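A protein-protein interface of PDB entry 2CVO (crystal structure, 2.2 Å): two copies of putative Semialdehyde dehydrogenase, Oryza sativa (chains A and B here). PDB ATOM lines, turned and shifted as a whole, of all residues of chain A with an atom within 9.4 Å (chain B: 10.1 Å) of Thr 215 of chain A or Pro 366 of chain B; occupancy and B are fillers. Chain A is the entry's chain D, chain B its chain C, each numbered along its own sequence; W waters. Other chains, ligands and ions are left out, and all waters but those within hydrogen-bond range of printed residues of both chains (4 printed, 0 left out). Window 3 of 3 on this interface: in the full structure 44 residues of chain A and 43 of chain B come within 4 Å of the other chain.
Water W2 lies within hydrogen-bond range of the side-chain hydroxyl (OG1) of Thr 304 of chain B (2.6 Å), the backbone carbonyl oxygen (O) of Glu 219 of chain A (2.8 Å) and the backbone NH (N) of Arg 305 of chain B (3.5 Å). Water W4 lies within hydrogen-bond range of O of Thr 215 of chain A, O of Ala 218 of chain A and NH1 of Arg 305 of chain B. Water W3 bridges a ring nitrogen (NE2) of His 306 of chain B (2.7 Å) and the side-chain carboxylate of Glu 216 of chain A (2.9 Å). Water W1 lies within hydrogen-bond range of the backbone carbonyl oxygen of Gly 220 of chain A (2.7 Å) and the guanidinium group of Arg 305 of chain B (3.0 Å).
Of the printed residues of chain B, Thr 215 of chain A touches Phe 365 (3.7 Å) and Pro 366 (3.98 Å). Of chain B, only Arg 305 (3.2 Å) and Phe 365 (3.5 Å) come within 4 Å of Glu 216 of chain A. Printed residues of chain B within 4 Å of Glu 219 of chain A: Lys 259 (2.7 Å). Of the printed residues of chain A, Thr 304 of chain B touches Gly 220 (3.4 Å). Leu 364 of chain B touches none of the printed residues of chain A. Of the printed residues of chain A, Phe 365 of chain B touches Thr 215 and Glu 216. Of the printed residues of chain A, Pro 366 of chain B touches Thr 215 (3.98 Å). The nearest printed residue of chain B that does not touch Thr 215 of chain A is Arg 305 of chain B (5.5 Å). The nearest printed residue of chain B that does not touch Glu 219 of chain A is Arg 305 of chain B (4.3 Å).
Of the 13 printed residues of chain A, 6 touch a printed residue of chain B. Printed residues of chain A that touch a printed residue of chain B: Thr 215, Glu 216, Ile 217, Ala 218, Glu 219 and Gly 220. Of the 13 printed residues of chain B, 5 touch a printed residue of chain A. Printed residues of chain B that touch a printed residue of chain A: Lys 259, Thr 304, Arg 305, Phe 365 and Pro 366. Hydrophobic or aromatic side chains of chain B within 4 Å of the printed part of chain A: Phe 365 and Pro 366. Along chain B the printed residues that touch a printed residue of chain A span positions 259 to 366. Among the printed residues, no Asp or Glu carboxylate lies within 4 Å of a Lys or Arg side-chain nitrogen of the other chain.
Thr 215 of chain A touches Phe 365 of chain B. Thr 215 of chain A touches Pro 366 of chain B (O to CB, 3.98 Å). Phe 365 of chain B touches Glu 216 of chain A (CZ to OE1, 3.5 Å). Arg 305 of chain B touches Ala 218 of chain A (NH1 to O, 3.9 Å). Gly 220 of chain A touches Thr 304 of chain B.
The backbone carbonyl oxygen of Gly 220 of chain A lies within hydrogen-bond range of the side-chain sulfur of Cys 257 of chain A (3.4 Å). A ring nitrogen (ND1) of His 303 of chain B lies within hydrogen-bond range of the guanidinium group (NE) of Arg 305 of chain B (3.1 Å).
The guanidinium group of Arg 305 of chain B sits at hydrogen-bond distance from the backbone carbonyl oxygen of Glu 216 of chain A. The guanidinium group (NH1) of Arg 305 of chain B is in hydrogen-bond range of the backbone carbonyl oxygen (O) of Ile 217 of chain A, at 2.8 Å. The backbone NH of Lys 259 of chain B sits at hydrogen-bond distance from the side-chain carboxylate of Glu 219 of chain A, at 2.7 Å. NH2 of Arg 305 of chain B is in hydrogen-bond range of O of Gly 220 of chain A (3.4 Å).
No position is printed for both chains. Of the 9 pairs that touch across the chains among the printed residues, none has its exchanged pair printed and touching as well.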
ATOM      1  N   LYS A 209      10.615  28.732  -6.261  1.00  0.00           N
ATOM      2  CA  LYS A 209      10.476  29.946  -7.053  1.00  0.00           C
ATOM      3  C   LYS A 209       9.771  29.613  -8.353  1.00  0.00           C
ATOM      4  O   LYS A 209       9.992  28.549  -8.931  1.00  0.00           O
ATOM      5  CB  LYS A 209      11.845  30.556  -7.378  1.00  0.00           C
ATOM      6  CG  LYS A 209      12.646  31.005  -6.172  1.00  0.00           C
ATOM      7  CD  LYS A 209      13.926  31.700  -6.602  1.00  0.00           C
ATOM      8  CE  LYS A 209      14.866  31.910  -5.424  1.00  0.00           C
ATOM      9  NZ  LYS A 209      15.324  30.613  -4.844  1.00  0.00           N
ATOM     10  N   GLU A 210       8.931  30.530  -8.811  1.00  0.00           N
ATOM     11  CA  GLU A 210       8.200  30.339 -10.055  1.00  0.00           C
ATOM     12  C   GLU A 210       9.176  30.221 -11.222  1.00  0.00           C
ATOM     13  O   GLU A 210       9.032  29.355 -12.078  1.00  0.00           O
ATOM     14  CB  GLU A 210       7.260  31.521 -10.291  1.00  0.00           C
ATOM     15  CG  GLU A 210       6.606  31.528 -11.658  1.00  0.00           C
ATOM     16  CD  GLU A 210       5.830  32.805 -11.930  1.00  0.00           C
ATOM     17  OE1 GLU A 210       4.781  33.025 -11.286  1.00  0.00           O
ATOM     18  OE2 GLU A 210       6.278  33.593 -12.787  1.00  0.00           O
ATOM     19  N   ALA A 211      10.176  31.094 -11.237  1.00  0.00           N
ATOM     20  CA  ALA A 211      11.170  31.122 -12.306  1.00  0.00           C
ATOM     21  C   ALA A 211      11.938  29.819 -12.540  1.00  0.00           C
ATOM     22  O   ALA A 211      12.399  29.570 -13.649  1.00  0.00           O
ATOM     23  CB  ALA A 211      12.164  32.259 -12.054  1.00  0.00           C
ATOM     24  N   ASN A 212      12.071  28.988 -11.511  1.00  0.00           N
ATOM     25  CA  ASN A 212      12.833  27.750 -11.653  1.00  0.00           C
ATOM     26  C   ASN A 212      12.024  26.470 -11.821  1.00  0.00           C
ATOM     27  O   ASN A 212      12.580  25.368 -11.791  1.00  0.00           O
ATOM     28  CB  ASN A 212      13.797  27.627 -10.478  1.00  0.00           C
ATOM     29  CG  ASN A 212      14.790  28.785 -10.427  1.00  0.00           C
ATOM     30  OD1 ASN A 212      15.230  29.205  -9.352  1.00  0.00           O
ATOM     31  ND2 ASN A 212      15.149  29.299 -11.593  1.00  0.00           N
ATOM     32  N   LEU A 213      10.717  26.623 -12.008  1.00  0.00           N
ATOM     33  CA  LEU A 213       9.814  25.493 -12.224  1.00  0.00           C
ATOM     34  C   LEU A 213      10.211  24.755 -13.499  1.00  0.00           C
ATOM     35  O   LEU A 213      10.781  25.350 -14.417  1.00  0.00           O
ATOM     36  CB  LEU A 213       8.367  25.983 -12.367  1.00  0.00           C
ATOM     37  CG  LEU A 213       7.634  26.424 -11.097  1.00  0.00           C
ATOM     38  CD1 LEU A 213       6.305  27.108 -11.454  1.00  0.00           C
ATOM     39  CD2 LEU A 213       7.401  25.202 -10.219  1.00  0.00           C
ATOM     40  N   TYR A 214       9.916  23.462 -13.557  1.00  0.00           N
ATOM     41  CA  TYR A 214      10.239  22.677 -14.742  1.00  0.00           C
ATOM     42  C   TYR A 214       9.579  23.308 -15.964  1.00  0.00           C
ATOM     43  O   TYR A 214      10.179  23.385 -17.037  1.00  0.00           O
ATOM     44  CB  TYR A 214       9.739  21.237 -14.605  1.00  0.00           C
ATOM     45  CG  TYR A 214      10.073  20.384 -15.812  1.00  0.00           C
ATOM     46  CD1 TYR A 214      11.284  19.698 -15.893  1.00  0.00           C
ATOM     47  CD2 TYR A 214       9.200  20.308 -16.897  1.00  0.00           C
ATOM     48  CE1 TYR A 214      11.624  18.957 -17.027  1.00  0.00           C
ATOM     49  CE2 TYR A 214       9.530  19.574 -18.040  1.00  0.00           C
ATOM     50  CZ  TYR A 214      10.745  18.905 -18.097  1.00  0.00           C
ATOM     51  OH  TYR A 214      11.090  18.212 -19.229  1.00  0.00           O
ATOM     52  N   THR A 215       8.337  23.752 -15.795  1.00  0.00           N
ATOM     53  CA  THR A 215       7.586  24.370 -16.886  1.00  0.00           C
ATOM     54  C   THR A 215       8.158  25.712 -17.347  1.00  0.00           C
ATOM     55  O   THR A 215       8.057  26.069 -18.524  1.00  0.00           O
ATOM     56  CB  THR A 215       6.111  24.585 -16.482  1.00  0.00           C
ATOM     57  OG1 THR A 215       6.062  25.188 -15.183  1.00  0.00           O
ATOM     58  CG2 THR A 215       5.355  23.254 -16.452  1.00  0.00           C
ATOM     59  N   GLU A 216       8.752  26.461 -16.424  1.00  0.00           N
ATOM     60  CA  GLU A 216       9.319  27.766 -16.759  1.00  0.00           C
ATOM     61  C   GLU A 216      10.758  27.656 -17.269  1.00  0.00           C
ATOM     62  O   GLU A 216      11.305  28.611 -17.817  1.00  0.00           O
ATOM     63  CB  GLU A 216       9.300  28.672 -15.526  1.00  0.00           C
ATOM     64  CG  GLU A 216       7.924  28.939 -14.937  1.00  0.00           C
ATOM     65  CD  GLU A 216       7.063  29.821 -15.825  1.00  0.00           C
ATOM     66  OE1 GLU A 216       7.567  30.855 -16.298  1.00  0.00           O
ATOM     67  OE2 GLU A 216       5.879  29.489 -16.039  1.00  0.00           O
ATOM     68  N   ILE A 217      11.360  26.485 -17.097  1.00  0.00           N
ATOM     69  CA  ILE A 217      12.748  26.269 -17.504  1.00  0.00           C
ATOM     70  C   ILE A 217      12.965  25.330 -18.689  1.00  0.00           C
ATOM     71  O   ILE A 217      13.762  25.622 -19.580  1.00  0.00           O
ATOM     72  CB  ILE A 217      13.584  25.714 -16.311  1.00  0.00           C
ATOM     73  CG1 ILE A 217      13.765  26.794 -15.237  1.00  0.00           C
ATOM     74  CG2 ILE A 217      14.931  25.205 -16.801  1.00  0.00           C
ATOM     75  CD1 ILE A 217      14.571  28.004 -15.698  1.00  0.00           C
ATOM     76  N   ALA A 218      12.268  24.201 -18.692  1.00  0.00           N
ATOM     77  CA  ALA A 218      12.439  23.202 -19.745  1.00  0.00           C
ATOM     78  C   ALA A 218      12.216  23.701 -21.171  1.00  0.00           C
ATOM     79  O   ALA A 218      11.334  24.518 -21.427  1.00  0.00           O
ATOM     80  CB  ALA A 218      11.534  21.995 -19.465  1.00  0.00           C
ATOM     81  N   GLU A 219      13.031  23.191 -22.090  1.00  0.00           N
ATOM     82  CA  GLU A 219      12.945  23.530 -23.509  1.00  0.00           C
ATOM     83  C   GLU A 219      13.140  25.007 -23.824  1.00  0.00           C
ATOM     84  O   GLU A 219      12.462  25.560 -24.694  1.00  0.00           O
ATOM     85  CB  GLU A 219      11.605  23.048 -24.089  1.00  0.00           C
ATOM     86  CG  GLU A 219      11.457  21.527 -24.122  1.00  0.00           C
ATOM     87  CD  GLU A 219      12.508  20.847 -25.000  1.00  0.00           C
ATOM     88  OE1 GLU A 219      12.601  21.185 -26.199  1.00  0.00           O
ATOM     89  OE2 GLU A 219      13.243  19.972 -24.493  1.00  0.00           O
ATOM     90  N   GLY A 220      14.082  25.640 -23.133  1.00  0.00           N
ATOM     91  CA  GLY A 220      14.349  27.045 -23.376  1.00  0.00           C
ATOM     92  C   GLY A 220      15.527  27.553 -22.571  1.00  0.00           C
ATOM     93  O   GLY A 220      15.918  26.928 -21.583  1.00  0.00           O
ATOM     94  N   CYS A 257      18.446  24.832 -19.783  1.00  0.00           N
ATOM     95  CA  CYS A 257      17.453  23.838 -19.409  1.00  0.00           C
ATOM     96  C   CYS A 257      18.076  22.458 -19.194  1.00  0.00           C
ATOM     97  O   CYS A 257      17.842  21.526 -19.967  1.00  0.00           O
ATOM     98  CB  CYS A 257      16.348  23.760 -20.470  1.00  0.00           C
ATOM     99  SG  CYS A 257      16.940  23.757 -22.174  1.00  0.00           S
ATOM    100  N   LYS B 259      14.471  21.093 -28.162  1.00  0.00           N
ATOM    101  CA  LYS B 259      14.114  20.868 -29.551  1.00  0.00           C
ATOM    102  C   LYS B 259      14.059  22.159 -30.361  1.00  0.00           C
ATOM    103  O   LYS B 259      14.774  22.293 -31.350  1.00  0.00           O
ATOM    104  CB  LYS B 259      12.778  20.113 -29.623  1.00  0.00           C
ATOM    105  CG  LYS B 259      12.826  18.764 -28.896  1.00  0.00           C
ATOM    106  CD  LYS B 259      11.580  17.918 -29.111  1.00  0.00           C
ATOM    107  CE  LYS B 259      10.366  18.499 -28.412  1.00  0.00           C
ATOM    108  NZ  LYS B 259       9.148  17.725 -28.748  1.00  0.00           N
ATOM    109  N   HIS B 303      13.581  35.373 -23.930  1.00  0.00           N
ATOM    110  CA  HIS B 303      13.778  33.951 -23.649  1.00  0.00           C
ATOM    111  C   HIS B 303      13.420  33.212 -24.932  1.00  0.00           C
ATOM    112  O   HIS B 303      12.454  33.575 -25.595  1.00  0.00           O
ATOM    113  CB  HIS B 303      12.837  33.453 -22.544  1.00  0.00           C
ATOM    114  CG  HIS B 303      13.136  33.996 -21.180  1.00  0.00           C
ATOM    115  ND1 HIS B 303      12.885  33.278 -20.029  1.00  0.00           N
ATOM    116  CD2 HIS B 303      13.620  35.195 -20.777  1.00  0.00           C
ATOM    117  CE1 HIS B 303      13.201  34.012 -18.977  1.00  0.00           C
ATOM    118  NE2 HIS B 303      13.650  35.178 -19.403  1.00  0.00           N
ATOM    119  N   THR B 304      14.183  32.185 -25.301  1.00  0.00           N
ATOM    120  CA  THR B 304      13.839  31.440 -26.509  1.00  0.00           C
ATOM    121  C   THR B 304      12.483  30.748 -26.305  1.00  0.00           C
ATOM    122  O   THR B 304      11.744  30.515 -27.260  1.00  0.00           O
ATOM    123  CB  THR B 304      14.871  30.335 -26.839  1.00  0.00           C
ATOM    124  OG1 THR B 304      14.888  29.369 -25.779  1.00  0.00           O
ATOM    125  CG2 THR B 304      16.264  30.923 -27.027  1.00  0.00           C
ATOM    126  N   ARG B 305      12.168  30.421 -25.053  1.00  0.00           N
ATOM    127  CA  ARG B 305      10.924  29.729 -24.723  1.00  0.00           C
ATOM    128  C   ARG B 305       9.696  30.585 -25.000  1.00  0.00           C
ATOM    129  O   ARG B 305       8.587  30.064 -25.145  1.00  0.00           O
ATOM    130  CB  ARG B 305      10.924  29.321 -23.243  1.00  0.00           C
ATOM    131  CG  ARG B 305      10.614  30.475 -22.296  1.00  0.00           C
ATOM    132  CD  ARG B 305      10.874  30.131 -20.831  1.00  0.00           C
ATOM    133  NE  ARG B 305      12.278  30.283 -20.442  1.00  0.00           N
ATOM    134  CZ  ARG B 305      13.143  29.282 -20.336  1.00  0.00           C
ATOM    135  NH1 ARG B 305      12.751  28.038 -20.597  1.00  0.00           N
ATOM    136  NH2 ARG B 305      14.392  29.522 -19.943  1.00  0.00           N
ATOM    137  N   HIS B 306       9.896  31.895 -25.079  1.00  0.00           N
ATOM    138  CA  HIS B 306       8.794  32.817 -25.307  1.00  0.00           C
ATOM    139  C   HIS B 306       8.407  33.076 -26.762  1.00  0.00           C
ATOM    140  O   HIS B 306       7.491  33.847 -27.016  1.00  0.00           O
ATOM    141  CB  HIS B 306       9.087  34.139 -24.590  1.00  0.00           C
ATOM    142  CG  HIS B 306       9.075  34.022 -23.096  1.00  0.00           C
ATOM    143  ND1 HIS B 306       9.900  34.766 -22.280  1.00  0.00           N
ATOM    144  CD2 HIS B 306       8.349  33.227 -22.271  1.00  0.00           C
ATOM    145  CE1 HIS B 306       9.688  34.432 -21.019  1.00  0.00           C
ATOM    146  NE2 HIS B 306       8.751  33.500 -20.986  1.00  0.00           N
ATOM    147  N   VAL B 307       9.094  32.445 -27.713  1.00  0.00           N
ATOM    148  CA  VAL B 307       8.754  32.622 -29.127  1.00  0.00           C
ATOM    149  C   VAL B 307       8.581  31.268 -29.829  1.00  0.00           C
ATOM    150  O   VAL B 307       8.327  31.208 -31.037  1.00  0.00           O
ATOM    151  CB  VAL B 307       9.825  33.451 -29.887  1.00  0.00           C
ATOM    152  CG1 VAL B 307       9.954  34.845 -29.257  1.00  0.00           C
ATOM    153  CG2 VAL B 307      11.159  32.722 -29.872  1.00  0.00           C
ATOM    154  N   VAL B 308       8.722  30.186 -29.067  1.00  0.00           N
ATOM    155  CA  VAL B 308       8.574  28.838 -29.607  1.00  0.00           C
ATOM    156  C   VAL B 308       7.223  28.668 -30.306  1.00  0.00           C
ATOM    157  O   VAL B 308       6.174  28.974 -29.738  1.00  0.00           O
ATOM    158  CB  VAL B 308       8.692  27.775 -28.481  1.00  0.00           C
ATOM    159  CG1 VAL B 308       8.140  26.433 -28.959  1.00  0.00           C
ATOM    160  CG2 VAL B 308      10.152  27.622 -28.057  1.00  0.00           C
ATOM    161  N   GLY B 309       7.255  28.182 -31.542  1.00  0.00           N
ATOM    162  CA  GLY B 309       6.022  27.973 -32.275  1.00  0.00           C
ATOM    163  C   GLY B 309       5.428  29.228 -32.884  1.00  0.00           C
ATOM    164  O   GLY B 309       4.317  29.189 -33.406  1.00  0.00           O
ATOM    165  N   GLN B 362       0.150  32.371 -31.667  1.00  0.00           N
ATOM    166  CA  GLN B 362       0.909  32.876 -30.539  1.00  0.00           C
ATOM    167  C   GLN B 362       1.784  31.752 -29.988  1.00  0.00           C
ATOM    168  O   GLN B 362       1.417  30.581 -30.044  1.00  0.00           O
ATOM    169  CB  GLN B 362      -0.031  33.413 -29.468  1.00  0.00           C
ATOM    170  CG  GLN B 362      -0.698  34.726 -29.863  1.00  0.00           C
ATOM    171  CD  GLN B 362       0.315  35.782 -30.277  1.00  0.00           C
ATOM    172  OE1 GLN B 362       0.483  36.072 -31.467  1.00  0.00           O
ATOM    173  NE2 GLN B 362       1.006  36.350 -29.297  1.00  0.00           N
ATOM    174  N   PRO B 363       2.955  32.102 -29.443  1.00  0.00           N
ATOM    175  CA  PRO B 363       3.874  31.104 -28.893  1.00  0.00           C
ATOM    176  C   PRO B 363       3.260  30.080 -27.950  1.00  0.00           C
ATOM    177  O   PRO B 363       2.397  30.396 -27.131  1.00  0.00           O
ATOM    178  CB  PRO B 363       4.967  31.953 -28.235  1.00  0.00           C
ATOM    179  CG  PRO B 363       4.301  33.281 -27.998  1.00  0.00           C
ATOM    180  CD  PRO B 363       3.449  33.470 -29.209  1.00  0.00           C
ATOM    181  N   LEU B 364       3.712  28.839 -28.087  1.00  0.00           N
ATOM    182  CA  LEU B 364       3.220  27.755 -27.254  1.00  0.00           C
ATOM    183  C   LEU B 364       4.043  27.677 -25.976  1.00  0.00           C
ATOM    184  O   LEU B 364       5.105  27.058 -25.942  1.00  0.00           O
ATOM    185  CB  LEU B 364       3.302  26.420 -28.001  1.00  0.00           C
ATOM    186  CG  LEU B 364       2.533  25.271 -27.341  1.00  0.00           C
ATOM    187  CD1 LEU B 364       1.037  25.563 -27.416  1.00  0.00           C
ATOM    188  CD2 LEU B 364       2.842  23.963 -28.035  1.00  0.00           C
ATOM    189  N   PHE B 365       3.555  28.331 -24.931  1.00  0.00           N
ATOM    190  CA  PHE B 365       4.226  28.315 -23.642  1.00  0.00           C
ATOM    191  C   PHE B 365       3.143  28.194 -22.576  1.00  0.00           C
ATOM    192  O   PHE B 365       2.121  28.864 -22.655  1.00  0.00           O
ATOM    193  CB  PHE B 365       5.015  29.608 -23.418  1.00  0.00           C
ATOM    194  CG  PHE B 365       5.627  29.698 -22.051  1.00  0.00           C
ATOM    195  CD1 PHE B 365       6.856  29.102 -21.784  1.00  0.00           C
ATOM    196  CD2 PHE B 365       4.928  30.287 -21.003  1.00  0.00           C
ATOM    197  CE1 PHE B 365       7.378  29.086 -20.495  1.00  0.00           C
ATOM    198  CE2 PHE B 365       5.438  30.277 -19.710  1.00  0.00           C
ATOM    199  CZ  PHE B 365       6.666  29.673 -19.455  1.00  0.00           C
ATOM    200  N   PRO B 366       3.347  27.329 -21.572  1.00  0.00           N
ATOM    201  CA  PRO B 366       4.519  26.468 -21.389  1.00  0.00           C
ATOM    202  C   PRO B 366       4.548  25.332 -22.410  1.00  0.00           C
ATOM    203  O   PRO B 366       3.604  25.253 -23.224  1.00  0.00           O
ATOM    204  CB  PRO B 366       4.343  25.960 -19.962  1.00  0.00           C
ATOM    205  CG  PRO B 366       2.864  25.849 -19.841  1.00  0.00           C
ATOM    206  CD  PRO B 366       2.382  27.139 -20.475  1.00  0.00           C
ATOM    207  OXT PRO B 366       5.514  24.543 -22.387  1.00  0.00           O
HETATM  208  O   HOH W   1      16.546  27.723 -19.028  1.00  0.00           O
HETATM  209  O   HOH W   2      13.329  27.489 -26.530  1.00  0.00           O
HETATM  210  O   HOH W   3       7.632  32.574 -18.653  1.00  0.00           O
HETATM  211  O   HOH W   4       9.687  26.709 -20.513  1.00  0.00           O
